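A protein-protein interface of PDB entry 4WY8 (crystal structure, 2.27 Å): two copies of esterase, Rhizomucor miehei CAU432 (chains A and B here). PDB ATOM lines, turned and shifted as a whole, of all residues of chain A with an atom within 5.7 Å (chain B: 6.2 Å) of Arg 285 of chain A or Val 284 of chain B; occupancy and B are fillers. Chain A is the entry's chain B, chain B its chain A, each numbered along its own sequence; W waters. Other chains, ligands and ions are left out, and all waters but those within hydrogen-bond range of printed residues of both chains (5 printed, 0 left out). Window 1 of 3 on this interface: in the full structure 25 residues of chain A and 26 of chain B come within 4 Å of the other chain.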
ATOM      1  N   VAL A 255     -11.922 -11.008   5.028  1.00  0.00           N
ATOM      2  CA  VAL A 255     -11.695  -9.872   4.150  1.00  0.00           C
ATOM      3  C   VAL A 255     -10.966  -8.771   4.907  1.00  0.00           C
ATOM      4  O   VAL A 255     -11.469  -8.223   5.887  1.00  0.00           O
ATOM      5  CB  VAL A 255     -13.016  -9.312   3.571  1.00  0.00           C
ATOM      6  CG1 VAL A 255     -12.721  -8.219   2.564  1.00  0.00           C
ATOM      7  CG2 VAL A 255     -13.821 -10.420   2.903  1.00  0.00           C
ATOM      8  N   ILE A 256      -9.755  -8.475   4.457  1.00  0.00           N
ATOM      9  CA  ILE A 256      -8.903  -7.513   5.125  1.00  0.00           C
ATOM     10  C   ILE A 256      -8.732  -6.304   4.224  1.00  0.00           C
ATOM     11  O   ILE A 256      -8.380  -6.463   3.055  1.00  0.00           O
ATOM     12  CB  ILE A 256      -7.532  -8.125   5.456  1.00  0.00           C
ATOM     13  CG1 ILE A 256      -7.696  -9.270   6.459  1.00  0.00           C
ATOM     14  CG2 ILE A 256      -6.584  -7.063   6.044  1.00  0.00           C
ATOM     15  CD1 ILE A 256      -6.518 -10.238   6.472  1.00  0.00           C
ATOM     16  N   THR A 257      -9.026  -5.109   4.745  1.00  0.00           N
ATOM     17  CA  THR A 257      -8.838  -3.877   3.975  1.00  0.00           C
ATOM     18  C   THR A 257      -7.859  -2.952   4.672  1.00  0.00           C
ATOM     19  O   THR A 257      -7.691  -3.028   5.883  1.00  0.00           O
ATOM     20  CB  THR A 257     -10.149  -3.098   3.773  1.00  0.00           C
ATOM     21  OG1 THR A 257     -10.788  -2.903   5.048  1.00  0.00           O
ATOM     22  CG2 THR A 257     -11.073  -3.846   2.834  1.00  0.00           C
ATOM     23  N   ALA A 258      -7.239  -2.066   3.904  1.00  0.00           N
ATOM     24  CA  ALA A 258      -6.335  -1.078   4.469  1.00  0.00           C
ATOM     25  C   ALA A 258      -7.061   0.249   4.570  1.00  0.00           C
ATOM     26  O   ALA A 258      -7.855   0.600   3.697  1.00  0.00           O
ATOM     27  CB  ALA A 258      -5.085  -0.937   3.619  1.00  0.00           C
ATOM     28  N   GLU A 259      -6.800   0.994   5.631  1.00  0.00           N
ATOM     29  CA  GLU A 259      -7.450   2.288   5.774  1.00  0.00           C
ATOM     30  C   GLU A 259      -7.091   3.274   4.634  1.00  0.00           C
ATOM     31  O   GLU A 259      -7.979   3.946   4.087  1.00  0.00           O
ATOM     32  CB  GLU A 259      -7.090   2.911   7.133  1.00  0.00           C
ATOM     33  CG  GLU A 259      -7.829   4.211   7.410  1.00  0.00           C
ATOM     34  CD  GLU A 259      -7.341   4.926   8.656  1.00  0.00           C
ATOM     35  OE1 GLU A 259      -6.130   4.828   8.956  1.00  0.00           O
ATOM     36  OE2 GLU A 259      -8.173   5.594   9.323  1.00  0.00           O
ATOM     37  N   ARG A 264     -10.292   0.448  -0.725  1.00  0.00           N
ATOM     38  CA  ARG A 264     -10.901   0.195   0.579  1.00  0.00           C
ATOM     39  C   ARG A 264     -12.432   0.033   0.510  1.00  0.00           C
ATOM     40  O   ARG A 264     -12.999  -0.924   1.077  1.00  0.00           O
ATOM     41  CB  ARG A 264     -10.539   1.310   1.556  1.00  0.00           C
ATOM     42  CG  ARG A 264     -11.104   1.060   2.950  1.00  0.00           C
ATOM     43  CD  ARG A 264     -10.824   2.224   3.877  1.00  0.00           C
ATOM     44  NE  ARG A 264     -11.699   3.344   3.544  1.00  0.00           N
ATOM     45  CZ  ARG A 264     -11.468   4.604   3.893  1.00  0.00           C
ATOM     46  NH1 ARG A 264     -10.393   4.920   4.615  1.00  0.00           N
ATOM     47  NH2 ARG A 264     -12.335   5.543   3.546  1.00  0.00           N
ATOM     48  N   GLU A 265     -13.095   0.961  -0.183  1.00  0.00           N
ATOM     49  CA  GLU A 265     -14.559   0.970  -0.227  1.00  0.00           C
ATOM     50  C   GLU A 265     -15.157  -0.239  -0.936  1.00  0.00           C
ATOM     51  O   GLU A 265     -16.145  -0.794  -0.463  1.00  0.00           O
ATOM     52  CB  GLU A 265     -15.059   2.264  -0.879  1.00  0.00           C
ATOM     53  CG  GLU A 265     -14.865   3.486   0.022  1.00  0.00           C
ATOM     54  CD  GLU A 265     -15.408   3.248   1.437  1.00  0.00           C
ATOM     55  OE1 GLU A 265     -16.573   2.791   1.550  1.00  0.00           O
ATOM     56  OE2 GLU A 265     -14.667   3.479   2.436  1.00  0.00           O
ATOM     57  N   GLU A 268     -14.685  -3.388   1.299  1.00  0.00           N
ATOM     58  CA  GLU A 268     -15.708  -3.418   2.343  1.00  0.00           C
ATOM     59  C   GLU A 268     -17.133  -3.628   1.785  1.00  0.00           C
ATOM     60  O   GLU A 268     -17.931  -4.346   2.389  1.00  0.00           O
ATOM     61  CB  GLU A 268     -15.599  -2.144   3.180  1.00  0.00           C
ATOM     62  CG  GLU A 268     -14.226  -2.121   3.890  1.00  0.00           C
ATOM     63  CD  GLU A 268     -14.020  -0.991   4.888  1.00  0.00           C
ATOM     64  OE1 GLU A 268     -14.924  -0.148   5.088  1.00  0.00           O
ATOM     65  OE2 GLU A 268     -12.923  -0.960   5.497  1.00  0.00           O
ATOM     66  N   ALA A 283     -14.688  -9.325   8.317  1.00  0.00           N
ATOM     67  CA  ALA A 283     -14.181  -8.209   7.540  1.00  0.00           C
ATOM     68  C   ALA A 283     -13.546  -7.224   8.502  1.00  0.00           C
ATOM     69  O   ALA A 283     -14.189  -6.786   9.456  1.00  0.00           O
ATOM     70  CB  ALA A 283     -15.295  -7.546   6.753  1.00  0.00           C
ATOM     71  N   VAL A 284     -12.279  -6.902   8.274  1.00  0.00           N
ATOM     72  CA  VAL A 284     -11.546  -6.030   9.183  1.00  0.00           C
ATOM     73  C   VAL A 284     -10.808  -4.980   8.376  1.00  0.00           C
ATOM     74  O   VAL A 284     -10.213  -5.279   7.329  1.00  0.00           O
ATOM     75  CB  VAL A 284     -10.512  -6.799  10.067  1.00  0.00           C
ATOM     76  CG1 VAL A 284     -11.204  -7.824  10.941  1.00  0.00           C
ATOM     77  CG2 VAL A 284      -9.514  -7.516   9.188  1.00  0.00           C
ATOM     78  N   ARG A 285     -10.864  -3.748   8.862  1.00  0.00           N
ATOM     79  CA  ARG A 285     -10.097  -2.663   8.288  1.00  0.00           C
ATOM     80  C   ARG A 285      -8.940  -2.377   9.223  1.00  0.00           C
ATOM     81  O   ARG A 285      -9.162  -2.140  10.413  1.00  0.00           O
ATOM     82  CB  ARG A 285     -10.959  -1.417   8.113  1.00  0.00           C
ATOM     83  CG  ARG A 285     -10.161  -0.211   7.614  1.00  0.00           C
ATOM     84  CD  ARG A 285     -10.925   1.086   7.851  1.00  0.00           C
ATOM     85  NE  ARG A 285     -12.148   1.179   7.054  1.00  0.00           N
ATOM     86  CZ  ARG A 285     -12.870   2.293   6.929  1.00  0.00           C
ATOM     87  NH1 ARG A 285     -12.511   3.407   7.585  1.00  0.00           N
ATOM     88  NH2 ARG A 285     -13.965   2.280   6.184  1.00  0.00           N
ATOM     89  N   TYR A 286      -7.716  -2.459   8.719  1.00  0.00           N
ATOM     90  CA  TYR A 286      -6.554  -2.100   9.519  1.00  0.00           C
ATOM     91  C   TYR A 286      -6.234  -0.628   9.335  1.00  0.00           C
ATOM     92  O   TYR A 286      -6.078  -0.146   8.205  1.00  0.00           O
ATOM     93  CB  TYR A 286      -5.346  -2.931   9.136  1.00  0.00           C
ATOM     94  CG  TYR A 286      -5.236  -4.248   9.874  1.00  0.00           C
ATOM     95  CD1 TYR A 286      -6.010  -5.348   9.507  1.00  0.00           C
ATOM     96  CD2 TYR A 286      -4.350  -4.390  10.928  1.00  0.00           C
ATOM     97  CE1 TYR A 286      -5.895  -6.558  10.180  1.00  0.00           C
ATOM     98  CE2 TYR A 286      -4.215  -5.587  11.599  1.00  0.00           C
ATOM     99  CZ  TYR A 286      -4.995  -6.666  11.229  1.00  0.00           C
ATOM    100  OH  TYR A 286      -4.864  -7.850  11.912  1.00  0.00           O
ATOM    101  N   LEU A 287      -6.077   0.068  10.448  1.00  0.00           N
ATOM    102  CA  LEU A 287      -5.856   1.503  10.409  1.00  0.00           C
ATOM    103  C   LEU A 287      -4.381   1.833  10.251  1.00  0.00           C
ATOM    104  O   LEU A 287      -3.516   1.084  10.731  1.00  0.00           O
ATOM    105  CB  LEU A 287      -6.361   2.157  11.681  1.00  0.00           C
ATOM    106  CG  LEU A 287      -7.816   2.615  11.707  1.00  0.00           C
ATOM    107  CD1 LEU A 287      -8.777   1.419  11.756  1.00  0.00           C
ATOM    108  CD2 LEU A 287      -7.991   3.492  12.930  1.00  0.00           C
ATOM    109  N   LEU B 254      -3.280  -3.136  21.244  1.00  0.00           N
ATOM    110  CA  LEU B 254      -4.260  -3.607  20.260  1.00  0.00           C
ATOM    111  C   LEU B 254      -5.571  -2.877  20.524  1.00  0.00           C
ATOM    112  O   LEU B 254      -6.141  -2.992  21.606  1.00  0.00           O
ATOM    113  CB  LEU B 254      -4.437  -5.130  20.338  1.00  0.00           C
ATOM    114  CG  LEU B 254      -5.571  -5.788  19.521  1.00  0.00           C
ATOM    115  CD1 LEU B 254      -5.396  -5.556  18.022  1.00  0.00           C
ATOM    116  CD2 LEU B 254      -5.706  -7.313  19.828  1.00  0.00           C
ATOM    117  N   VAL B 255      -6.016  -2.090  19.546  1.00  0.00           N
ATOM    118  CA  VAL B 255      -7.229  -1.300  19.686  1.00  0.00           C
ATOM    119  C   VAL B 255      -8.244  -1.823  18.681  1.00  0.00           C
ATOM    120  O   VAL B 255      -8.002  -1.807  17.460  1.00  0.00           O
ATOM    121  CB  VAL B 255      -6.961   0.205  19.455  1.00  0.00           C
ATOM    122  CG1 VAL B 255      -8.237   1.052  19.712  1.00  0.00           C
ATOM    123  CG2 VAL B 255      -5.845   0.667  20.366  1.00  0.00           C
ATOM    124  N   ILE B 256      -9.354  -2.336  19.201  1.00  0.00           N
ATOM    125  CA  ILE B 256     -10.388  -2.931  18.355  1.00  0.00           C
ATOM    126  C   ILE B 256     -11.652  -2.094  18.408  1.00  0.00           C
ATOM    127  O   ILE B 256     -12.175  -1.824  19.496  1.00  0.00           O
ATOM    128  CB  ILE B 256     -10.690  -4.387  18.786  1.00  0.00           C
ATOM    129  CG1 ILE B 256      -9.472  -5.270  18.531  1.00  0.00           C
ATOM    130  CG2 ILE B 256     -11.857  -4.967  17.990  1.00  0.00           C
ATOM    131  CD1 ILE B 256      -9.511  -6.540  19.333  1.00  0.00           C
ATOM    132  N   THR B 257     -12.148  -1.675  17.248  1.00  0.00           N
ATOM    133  CA  THR B 257     -13.377  -0.870  17.225  1.00  0.00           C
ATOM    134  C   THR B 257     -14.477  -1.571  16.423  1.00  0.00           C
ATOM    135  O   THR B 257     -14.199  -2.450  15.566  1.00  0.00           O
ATOM    136  CB  THR B 257     -13.148   0.547  16.612  1.00  0.00           C
ATOM    137  OG1 THR B 257     -12.607   0.431  15.286  1.00  0.00           O
ATOM    138  CG2 THR B 257     -12.206   1.382  17.493  1.00  0.00           C
ATOM    139  N   ALA B 258     -15.724  -1.193  16.718  1.00  0.00           N
ATOM    140  CA  ALA B 258     -16.879  -1.721  16.007  1.00  0.00           C
ATOM    141  C   ALA B 258     -17.364  -0.709  14.988  1.00  0.00           C
ATOM    142  O   ALA B 258     -17.425   0.495  15.273  1.00  0.00           O
ATOM    143  CB  ALA B 258     -18.011  -2.079  16.996  1.00  0.00           C
ATOM    144  N   GLU B 268     -10.862   5.004  17.401  1.00  0.00           N
ATOM    145  CA  GLU B 268      -9.919   5.106  16.290  1.00  0.00           C
ATOM    146  C   GLU B 268      -8.993   6.351  16.392  1.00  0.00           C
ATOM    147  O   GLU B 268      -7.780   6.245  16.148  1.00  0.00           O
ATOM    148  CB  GLU B 268     -10.688   5.066  14.956  1.00  0.00           C
ATOM    149  CG  GLU B 268     -11.373   3.694  14.778  1.00  0.00           C
ATOM    150  CD  GLU B 268     -11.983   3.434  13.408  1.00  0.00           C
ATOM    151  OE1 GLU B 268     -11.907   4.304  12.514  1.00  0.00           O
ATOM    152  OE2 GLU B 268     -12.525   2.312  13.218  1.00  0.00           O
ATOM    153  N   THR B 282      -1.608  -1.742  17.051  1.00  0.00           N
ATOM    154  CA  THR B 282      -2.384  -2.426  16.025  1.00  0.00           C
ATOM    155  C   THR B 282      -3.834  -1.973  16.216  1.00  0.00           C
ATOM    156  O   THR B 282      -4.387  -2.141  17.299  1.00  0.00           O
ATOM    157  CB  THR B 282      -2.250  -3.969  16.150  1.00  0.00           C
ATOM    158  OG1 THR B 282      -0.865  -4.322  16.180  1.00  0.00           O
ATOM    159  CG2 THR B 282      -2.935  -4.703  14.998  1.00  0.00           C
ATOM    160  N   ALA B 283      -4.418  -1.333  15.201  1.00  0.00           N
ATOM    161  CA  ALA B 283      -5.789  -0.789  15.300  1.00  0.00           C
ATOM    162  C   ALA B 283      -6.640  -1.357  14.184  1.00  0.00           C
ATOM    163  O   ALA B 283      -6.285  -1.281  13.007  1.00  0.00           O
ATOM    164  CB  ALA B 283      -5.791   0.748  15.245  1.00  0.00           C
ATOM    165  N   VAL B 284      -7.745  -1.978  14.558  1.00  0.00           N
ATOM    166  CA  VAL B 284      -8.578  -2.666  13.579  1.00  0.00           C
ATOM    167  C   VAL B 284     -10.040  -2.378  13.835  1.00  0.00           C
ATOM    168  O   VAL B 284     -10.491  -2.387  14.975  1.00  0.00           O
ATOM    169  CB  VAL B 284      -8.325  -4.193  13.613  1.00  0.00           C
ATOM    170  CG1 VAL B 284      -6.887  -4.480  13.305  1.00  0.00           C
ATOM    171  CG2 VAL B 284      -8.603  -4.733  14.987  1.00  0.00           C
ATOM    172  N   ARG B 285     -10.779  -2.106  12.773  1.00  0.00           N
ATOM    173  CA  ARG B 285     -12.227  -1.932  12.856  1.00  0.00           C
ATOM    174  C   ARG B 285     -12.907  -3.193  12.328  1.00  0.00           C
ATOM    175  O   ARG B 285     -12.605  -3.623  11.218  1.00  0.00           O
ATOM    176  CB  ARG B 285     -12.666  -0.714  12.041  1.00  0.00           C
ATOM    177  CG  ARG B 285     -14.181  -0.544  11.963  1.00  0.00           C
ATOM    178  CD  ARG B 285     -14.567   0.372  10.817  1.00  0.00           C
ATOM    179  NE  ARG B 285     -14.079   1.738  11.013  1.00  0.00           N
ATOM    180  CZ  ARG B 285     -14.489   2.780  10.294  1.00  0.00           C
ATOM    181  NH1 ARG B 285     -15.389   2.597   9.337  1.00  0.00           N
ATOM    182  NH2 ARG B 285     -13.999   3.996  10.526  1.00  0.00           N
ATOM    183  N   TYR B 286     -13.771  -3.821  13.124  1.00  0.00           N
ATOM    184  CA  TYR B 286     -14.516  -4.975  12.626  1.00  0.00           C
ATOM    185  C   TYR B 286     -15.816  -4.528  11.998  1.00  0.00           C
ATOM    186  O   TYR B 286     -16.575  -3.759  12.607  1.00  0.00           O
ATOM    187  CB  TYR B 286     -14.782  -5.978  13.744  1.00  0.00           C
ATOM    188  CG  TYR B 286     -13.658  -6.986  13.909  1.00  0.00           C
ATOM    189  CD1 TYR B 286     -12.452  -6.629  14.517  1.00  0.00           C
ATOM    190  CD2 TYR B 286     -13.811  -8.300  13.478  1.00  0.00           C
ATOM    191  CE1 TYR B 286     -11.409  -7.555  14.659  1.00  0.00           C
ATOM    192  CE2 TYR B 286     -12.787  -9.231  13.634  1.00  0.00           C
ATOM    193  CZ  TYR B 286     -11.596  -8.849  14.226  1.00  0.00           C
ATOM    194  OH  TYR B 286     -10.596  -9.775  14.381  1.00  0.00           O
ATOM    195  N   LEU B 287     -16.086  -5.011  10.789  1.00  0.00           N
ATOM    196  CA  LEU B 287     -17.293  -4.592  10.092  1.00  0.00           C
ATOM    197  C   LEU B 287     -18.505  -5.424  10.491  1.00  0.00           C
ATOM    198  O   LEU B 287     -18.377  -6.595  10.889  1.00  0.00           O
ATOM    199  CB  LEU B 287     -17.101  -4.653   8.584  1.00  0.00           C
ATOM    200  CG  LEU B 287     -16.648  -3.327   7.955  1.00  0.00           C
ATOM    201  CD1 LEU B 287     -15.188  -2.980   8.287  1.00  0.00           C
ATOM    202  CD2 LEU B 287     -16.864  -3.366   6.458  1.00  0.00           C
ATOM    203  N   HIS B 309      -8.343 -13.599  17.326  1.00  0.00           N
ATOM    204  CA  HIS B 309      -7.429 -12.529  16.959  1.00  0.00           C
ATOM    205  C   HIS B 309      -6.633 -11.987  18.148  1.00  0.00           C
ATOM    206  O   HIS B 309      -5.390 -11.906  18.111  1.00  0.00           O
ATOM    207  CB  HIS B 309      -8.221 -11.418  16.305  1.00  0.00           C
ATOM    208  CG  HIS B 309      -7.379 -10.307  15.790  1.00  0.00           C
ATOM    209  ND1 HIS B 309      -7.915  -9.202  15.173  1.00  0.00           N
ATOM    210  CD2 HIS B 309      -6.034 -10.140  15.780  1.00  0.00           C
ATOM    211  CE1 HIS B 309      -6.932  -8.397  14.795  1.00  0.00           C
ATOM    212  NE2 HIS B 309      -5.786  -8.941  15.157  1.00  0.00           N
HETATM  213  O   HOH W   1     -10.841   4.070  10.040  1.00  0.00           O
HETATM  214  O   HOH W   2     -16.394   0.629   7.798  1.00  0.00           O
HETATM  215  O   HOH W   3      -3.322  -1.162  12.315  1.00  0.00           O
HETATM  216  O   HOH W   4      -3.575  -8.000  14.548  1.00  0.00           O
HETATM  217  O   HOH W   5     -16.422  -8.552  10.611  1.00  0.00           O
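Water W4 bridges NE2 of His 309 of chain B (2.5 Å) and OH of Tyr 286 of chain A (2.9 Å).
Water W2 lies within hydrogen-bond range of NH1 of Arg 285 of chain B, OE1 of Glu 268 of chain A and NH2 of Arg 285 of chain A.
Water W1 lies within hydrogen-bond range of OE1 of Glu 268 of chain B, NH1 of Arg 285 of chain A, OE2 of Glu 259 of chain A and NH2 of Arg 285 of chain B.
Water W3 lies within hydrogen-bond range of O of Leu 287 of chain A and O of Ala 283 of chain B.
Water W5 lies within hydrogen-bond range of O of Leu 287 of chain B (2.8 Å) and N of Ala 283 of chain A (3.0 Å).
Glu 268 of chain A touches Leu 287 of chain B, and with the chains exchanged Leu 287 of chain A touches Glu 268 of chain B.
Ala 283 of chain A touches Leu 287 of chain B, and with the chains exchanged Leu 287 of chain A touches Ala 283 of chain B.
Val 284 of chain A touches Arg 285 of chain B, and with the chains exchanged Arg 285 of chain A touches Val 284 of chain B.
Val 284 of chain A touches Tyr 286 of chain B, and with the chains exchanged Tyr 286 of chain A touches Val 284 of chain B.
Positions printed for both chains: 255, 256, 257, 258, 268, 283, 284, 285, 286 and 287.
Of the 15 pairs that touch across the chains among the printed residues, 13 have their exchanged pair printed and touching as well.
N of Leu 287 of chain A lies within hydrogen-bond range of O of Ala 283 of chain B, 2.9 Å away.
N of Arg 285 of chain B lies within hydrogen-bond range of O of Arg 285 of chain A (2.9 Å).
The backbone NH of Leu 287 of chain B sits at hydrogen-bond distance from the backbone carbonyl oxygen of Ala 283 of chain A (2.9 Å).
O of Ala 283 of chain A touches O of Arg 285 of chain B, 3.95 Å away.
O of Ala 283 of chain A touches CA of Tyr 286 of chain B, at 3.7 Å.
Val 284 of chain A touches Arg 285 of chain B (CA to O, 3.3 Å).
CG1 of Val 284 of chain A touches CE2 of Tyr 286 of chain B, at 3.4 Å.
Arg 285 of chain A touches Val 284 of chain B.
Tyr 286 of chain A touches Thr 282 of chain B.
Tyr 286 of chain A touches Ala 283 of chain B (CA to O, 3.6 Å).
Val 284 of chain B touches Tyr 286 of chain A.
OH of Tyr 286 of chain A touches NE2 of His 309 of chain B, at 3.5 Å.
Glu 268 of chain B touches Leu 287 of chain A (CB to CD2, 3.7 Å).
O of Val 255 of chain A lies within hydrogen-bond range of N of Val 284 of chain A (2.8 Å).
The backbone NH (N) of Thr 257 of chain A sits at hydrogen-bond distance from the backbone carbonyl oxygen (O) of Val 284 of chain A.
The backbone NH of Val 255 of chain B sits at hydrogen-bond distance from the backbone carbonyl oxygen of Thr 282 of chain B (2.8 Å).
The side-chain carboxylate (OE2) of Glu 265 of chain A lies within salt-bridge range of the guanidinium group (NH2) of Arg 285 of chain A (3.997 Å).
The guanidinium group (NE) of Arg 285 of chain A is in salt-bridge range of the side-chain carboxylate (OE2) of Glu 268 of chain A, at 2.8 Å.
OH of Tyr 286 of chain B sits at hydrogen-bond distance from ND1 of His 309 of chain B, 2.9 Å away.
Arg 285 of chain A touches just these residues of chain B: Ala 283 (3.97 Å), Val 284 (3.3 Å) and Arg 285 (2.9 Å).
Val 284 of chain B touches two residues of chain A.
Printed residues of chain A within 4 Å of Thr 282 of chain B: Tyr 286.
Printed residues of chain B within 4 Å of Tyr 286 of chain A: Thr 282 (3.7 Å), Ala 283 (3.6 Å), Val 284 (3.4 Å) and His 309 (3.5 Å).
Of the printed residues of chain B, Leu 287 of chain A touches Glu 268 (3.7 Å) and Ala 283 (2.9 Å).
The nearest residue of chain B that does not touch Arg 285 of chain A is Leu 287 of chain B (4.4 Å).
The nearest residue of chain A that does not touch Val 284 of chain B is Leu 287 of chain A (4.5 Å).
Of the 13 printed residues of chain B, 8 touch a printed residue of chain A.
Hydrophobic or aromatic side chains of chain B within 4 Å of the printed part of chain A: Ala 283, Val 284, Tyr 286, Leu 287 and His 309.
Along chain B the printed residues that touch a printed residue of chain A span positions 268 to 309.
Among the printed residues, 15 pairs touch across the chains.
Among the printed residues, no Asp or Glu carboxylate lies within 4 Å of a Lys or Arg side-chain nitrogen of the other chain.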
